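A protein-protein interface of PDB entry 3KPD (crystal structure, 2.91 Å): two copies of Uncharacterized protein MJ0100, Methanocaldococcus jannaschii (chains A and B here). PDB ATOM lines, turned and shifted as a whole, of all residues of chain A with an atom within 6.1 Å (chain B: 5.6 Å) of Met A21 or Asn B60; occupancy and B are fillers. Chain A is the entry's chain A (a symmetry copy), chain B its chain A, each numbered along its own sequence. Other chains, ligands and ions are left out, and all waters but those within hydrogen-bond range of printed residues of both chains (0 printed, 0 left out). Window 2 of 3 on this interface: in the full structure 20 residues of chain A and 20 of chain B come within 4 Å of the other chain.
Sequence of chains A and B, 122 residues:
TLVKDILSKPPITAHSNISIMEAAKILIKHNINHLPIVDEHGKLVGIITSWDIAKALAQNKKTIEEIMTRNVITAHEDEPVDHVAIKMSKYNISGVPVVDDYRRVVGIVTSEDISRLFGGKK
O of Leu B57 sits close to SD of Met A21, at 3.4 Å.
The backbone NH of Met A21 sits close to the side-chain hydroxyl of Ser A19.
Among the printed residues, pairs that only touch across the chains: Met A21 with Asn B60 (3.6 Å), Lys A25 with Ala B58 (3.9 Å) and Ile A53 with Leu B57 (3.9 Å).
Of chain B, only Leu B57 and Asn B60 come within 4 Å of Met A21. Of the printed residues of chain B, Lys A25 touches Ala B58 (3.9 Å). Of the printed residues of chain B, Ile A53 touches Leu B57 (3.9 Å). Lys B55 touches none of the printed residues of chain A. Of the printed residues of chain A, Leu B57 touches Met A21 and Ile A53. Printed residues of chain A within 4 Å of Ala B58: Lys A25 (3.9 Å). Asn B60 touches one residue of chain A. The nearest residue of chain B that does not touch Met A21 is Ala B58 (4.7 Å). The nearest residue of chain A that does not touch Asn B60 is Lys A25 (5.6 Å).
Of the 8 printed residues of chain B, 3 touch a printed residue of chain A. Hydrophobic or aromatic side chains of chain B within 4 Å of the printed part of chain A: Leu B57. Of the 10 printed residues of chain A, 3 touch a printed residue of chain B. Among the printed residues, 4 pairs touch across the chains.
No position is printed for both chains.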
ATOM      1  N   SER A  19      -0.980 -14.945  22.478  1.00  0.00           N
ATOM      2  CA  SER A  19      -0.827 -14.922  23.932  1.00  0.00           C
ATOM      3  C   SER A  19       0.343 -15.778  24.427  1.00  0.00           C
ATOM      4  O   SER A  19       0.576 -16.885  23.929  1.00  0.00           O
ATOM      5  CB  SER A  19      -2.113 -15.395  24.611  1.00  0.00           C
ATOM      6  OG  SER A  19      -1.849 -15.813  25.945  1.00  0.00           O
ATOM      7  N   ILE A  20       1.049 -15.261  25.431  1.00  0.00           N
ATOM      8  CA  ILE A  20       2.116 -15.976  26.140  1.00  0.00           C
ATOM      9  C   ILE A  20       1.813 -17.469  26.249  1.00  0.00           C
ATOM     10  O   ILE A  20       2.670 -18.325  26.000  1.00  0.00           O
ATOM     11  CB  ILE A  20       2.267 -15.427  27.586  1.00  0.00           C
ATOM     12  CG1 ILE A  20       2.025 -13.908  27.646  1.00  0.00           C
ATOM     13  CG2 ILE A  20       3.599 -15.847  28.198  1.00  0.00           C
ATOM     14  CD1 ILE A  20       3.205 -13.043  27.228  1.00  0.00           C
ATOM     15  N   MET A  21       0.566 -17.752  26.612  1.00  0.00           N
ATOM     16  CA  MET A  21       0.108 -19.094  26.930  1.00  0.00           C
ATOM     17  C   MET A  21      -0.036 -19.941  25.666  1.00  0.00           C
ATOM     18  O   MET A  21       0.083 -21.168  25.708  1.00  0.00           O
ATOM     19  CB  MET A  21      -1.215 -19.016  27.696  1.00  0.00           C
ATOM     20  CG  MET A  21      -1.360 -20.041  28.814  1.00  0.00           C
ATOM     21  SD  MET A  21      -2.153 -21.585  28.317  1.00  0.00           S
ATOM     22  CE  MET A  21      -3.195 -21.869  29.752  1.00  0.00           C
ATOM     23  N   GLU A  22      -0.283 -19.279  24.545  1.00  0.00           N
ATOM     24  CA  GLU A  22      -0.348 -19.974  23.282  1.00  0.00           C
ATOM     25  C   GLU A  22       1.073 -20.361  22.850  1.00  0.00           C
ATOM     26  O   GLU A  22       1.329 -21.506  22.445  1.00  0.00           O
ATOM     27  CB  GLU A  22      -1.023 -19.084  22.252  1.00  0.00           C
ATOM     28  CG  GLU A  22      -1.496 -19.796  20.992  1.00  0.00           C
ATOM     29  CD  GLU A  22      -2.136 -18.819  20.001  1.00  0.00           C
ATOM     30  OE1 GLU A  22      -2.400 -19.212  18.841  1.00  0.00           O
ATOM     31  OE2 GLU A  22      -2.367 -17.649  20.390  1.00  0.00           O
ATOM     32  N   ALA A  23       1.995 -19.407  22.966  1.00  0.00           N
ATOM     33  CA  ALA A  23       3.394 -19.651  22.667  1.00  0.00           C
ATOM     34  C   ALA A  23       3.883 -20.880  23.422  1.00  0.00           C
ATOM     35  O   ALA A  23       4.474 -21.780  22.836  1.00  0.00           O
ATOM     36  CB  ALA A  23       4.227 -18.434  23.019  1.00  0.00           C
ATOM     37  N   ALA A  24       3.605 -20.909  24.722  1.00  0.00           N
ATOM     38  CA  ALA A  24       3.978 -22.021  25.586  1.00  0.00           C
ATOM     39  C   ALA A  24       3.485 -23.347  25.016  1.00  0.00           C
ATOM     40  O   ALA A  24       4.247 -24.320  24.929  1.00  0.00           O
ATOM     41  CB  ALA A  24       3.435 -21.806  26.984  1.00  0.00           C
ATOM     42  N   LYS A  25       2.217 -23.380  24.611  1.00  0.00           N
ATOM     43  CA  LYS A  25       1.650 -24.571  24.001  1.00  0.00           C
ATOM     44  C   LYS A  25       2.397 -24.893  22.711  1.00  0.00           C
ATOM     45  O   LYS A  25       2.647 -26.057  22.400  1.00  0.00           O
ATOM     46  CB  LYS A  25       0.156 -24.378  23.734  1.00  0.00           C
ATOM     47  CG  LYS A  25      -0.743 -24.612  24.949  1.00  0.00           C
ATOM     48  CD  LYS A  25      -2.223 -24.485  24.576  1.00  0.00           C
ATOM     49  CE  LYS A  25      -3.076 -24.340  25.827  1.00  0.00           C
ATOM     50  NZ  LYS A  25      -4.377 -23.662  25.560  1.00  0.00           N
ATOM     51  N   ILE A  26       2.776 -23.852  21.975  1.00  0.00           N
ATOM     52  CA  ILE A  26       3.540 -24.041  20.756  1.00  0.00           C
ATOM     53  C   ILE A  26       4.845 -24.745  21.060  1.00  0.00           C
ATOM     54  O   ILE A  26       5.078 -25.822  20.525  1.00  0.00           O
ATOM     55  CB  ILE A  26       3.736 -22.734  19.988  1.00  0.00           C
ATOM     56  CG1 ILE A  26       2.565 -22.542  19.019  1.00  0.00           C
ATOM     57  CG2 ILE A  26       5.052 -22.740  19.219  1.00  0.00           C
ATOM     58  CD1 ILE A  26       2.232 -21.073  18.738  1.00  0.00           C
ATOM     59  N   ILE A  53       8.833 -16.997  28.836  1.00  0.00           N
ATOM     60  CA  ILE A  53       7.546 -17.392  29.413  1.00  0.00           C
ATOM     61  C   ILE A  53       7.616 -17.258  30.935  1.00  0.00           C
ATOM     62  O   ILE A  53       6.656 -16.836  31.577  1.00  0.00           O
ATOM     63  CB  ILE A  53       7.093 -18.839  29.027  1.00  0.00           C
ATOM     64  CG1 ILE A  53       7.435 -19.208  27.566  1.00  0.00           C
ATOM     65  CG2 ILE A  53       5.615 -19.015  29.277  1.00  0.00           C
ATOM     66  CD1 ILE A  53       6.616 -18.507  26.480  1.00  0.00           C
ATOM     67  N   ILE A  64       3.198 -10.884  24.012  1.00  0.00           N
ATOM     68  CA  ILE A  64       4.415 -11.422  23.404  1.00  0.00           C
ATOM     69  C   ILE A  64       5.443 -10.320  23.134  1.00  0.00           C
ATOM     70  O   ILE A  64       6.627 -10.481  23.463  1.00  0.00           O
ATOM     71  CB  ILE A  64       4.104 -12.181  22.094  1.00  0.00           C
ATOM     72  CG1 ILE A  64       3.302 -13.464  22.380  1.00  0.00           C
ATOM     73  CG2 ILE A  64       5.393 -12.450  21.282  1.00  0.00           C
ATOM     74  CD1 ILE A  64       4.119 -14.698  22.780  1.00  0.00           C
ATOM     75  N   LYS B  55       5.791 -25.554  30.733  1.00  0.00           N
ATOM     76  CA  LYS B  55       4.967 -26.750  30.736  1.00  0.00           C
ATOM     77  C   LYS B  55       3.747 -26.492  31.654  1.00  0.00           C
ATOM     78  O   LYS B  55       2.611 -26.805  31.288  1.00  0.00           O
ATOM     79  CB  LYS B  55       5.789 -27.966  31.190  1.00  0.00           C
ATOM     80  CG  LYS B  55       5.114 -29.321  31.035  1.00  0.00           C
ATOM     81  CD  LYS B  55       5.469 -30.049  29.722  1.00  0.00           C
ATOM     82  CE  LYS B  55       6.659 -31.024  29.886  1.00  0.00           C
ATOM     83  NZ  LYS B  55       6.783 -32.044  28.782  1.00  0.00           N
ATOM     84  N   ALA B  56       3.985 -25.893  32.824  1.00  0.00           N
ATOM     85  CA  ALA B  56       2.922 -25.610  33.799  1.00  0.00           C
ATOM     86  C   ALA B  56       1.782 -24.746  33.246  1.00  0.00           C
ATOM     87  O   ALA B  56       0.607 -25.017  33.518  1.00  0.00           O
ATOM     88  CB  ALA B  56       3.503 -24.970  35.056  1.00  0.00           C
ATOM     89  N   LEU B  57       2.134 -23.703  32.492  1.00  0.00           N
ATOM     90  CA  LEU B  57       1.140 -22.884  31.804  1.00  0.00           C
ATOM     91  C   LEU B  57       0.454 -23.715  30.746  1.00  0.00           C
ATOM     92  O   LEU B  57      -0.759 -23.634  30.581  1.00  0.00           O
ATOM     93  CB  LEU B  57       1.772 -21.669  31.124  1.00  0.00           C
ATOM     94  CG  LEU B  57       1.630 -20.230  31.631  1.00  0.00           C
ATOM     95  CD1 LEU B  57       1.917 -19.291  30.467  1.00  0.00           C
ATOM     96  CD2 LEU B  57       0.251 -19.915  32.221  1.00  0.00           C
ATOM     97  N   ALA B  58       1.242 -24.524  30.047  1.00  0.00           N
ATOM     98  CA  ALA B  58       0.775 -25.236  28.872  1.00  0.00           C
ATOM     99  C   ALA B  58      -0.261 -26.286  29.193  1.00  0.00           C
ATOM    100  O   ALA B  58      -1.160 -26.516  28.402  1.00  0.00           O
ATOM    101  CB  ALA B  58       1.940 -25.858  28.137  1.00  0.00           C
ATOM    102  N   GLN B  59      -0.143 -26.926  30.347  1.00  0.00           N
ATOM    103  CA  GLN B  59      -1.052 -28.019  30.692  1.00  0.00           C
ATOM    104  C   GLN B  59      -1.851 -27.700  31.957  1.00  0.00           C
ATOM    105  O   GLN B  59      -2.471 -28.588  32.548  1.00  0.00           O
ATOM    106  CB  GLN B  59      -0.280 -29.333  30.866  1.00  0.00           C
ATOM    107  CG  GLN B  59       0.819 -29.597  29.832  1.00  0.00           C
ATOM    108  CD  GLN B  59       1.840 -30.628  30.308  1.00  0.00           C
ATOM    109  OE1 GLN B  59       2.156 -30.698  31.495  1.00  0.00           O
ATOM    110  NE2 GLN B  59       2.362 -31.422  29.383  1.00  0.00           N
ATOM    111  N   ASN B  60      -1.825 -26.427  32.358  1.00  0.00           N
ATOM    112  CA  ASN B  60      -2.529 -25.919  33.556  1.00  0.00           C
ATOM    113  C   ASN B  60      -2.166 -26.612  34.863  1.00  0.00           C
ATOM    114  O   ASN B  60      -2.964 -26.611  35.805  1.00  0.00           O
ATOM    115  CB  ASN B  60      -4.058 -25.901  33.370  1.00  0.00           C
ATOM    116  CG  ASN B  60      -4.495 -25.028  32.205  1.00  0.00           C
ATOM    117  OD1 ASN B  60      -4.671 -25.521  31.088  1.00  0.00           O
ATOM    118  ND2 ASN B  60      -4.659 -23.724  32.452  1.00  0.00           N
ATOM    119  N   LYS B  61      -0.962 -27.188  34.917  1.00  0.00           N
ATOM    120  CA  LYS B  61      -0.408 -27.756  36.151  1.00  0.00           C
ATOM    121  C   LYS B  61      -0.157 -26.652  37.201  1.00  0.00           C
ATOM    122  O   LYS B  61       0.069 -25.490  36.849  1.00  0.00           O
ATOM    123  CB  LYS B  61       0.857 -28.570  35.847  1.00  0.00           C
ATOM    124  CG  LYS B  61       0.708 -29.558  34.679  1.00  0.00           C
ATOM    125  CD  LYS B  61       0.125 -30.917  35.087  1.00  0.00           C
ATOM    126  CE  LYS B  61      -0.774 -31.489  33.976  1.00  0.00           C
ATOM    127  NZ  LYS B  61      -0.767 -32.979  33.892  1.00  0.00           N
ATOM    128  N   LYS B  62      -0.210 -27.009  38.482  1.00  0.00           N
ATOM    129  CA  LYS B  62      -0.329 -25.998  39.527  1.00  0.00           C
ATOM    130  C   LYS B  62       0.681 -26.114  40.664  1.00  0.00           C
ATOM    131  O   LYS B  62       0.878 -25.151  41.418  1.00  0.00           O
ATOM    132  CB  LYS B  62      -1.756 -25.998  40.092  1.00  0.00           C
ATOM    133  CG  LYS B  62      -2.299 -24.597  40.433  1.00  0.00           C
ATOM    134  CD  LYS B  62      -3.794 -24.652  40.798  1.00  0.00           C
ATOM    135  CE  LYS B  62      -4.510 -23.330  40.519  1.00  0.00           C
ATOM    136  NZ  LYS B  62      -4.714 -23.087  39.062  1.00  0.00           N
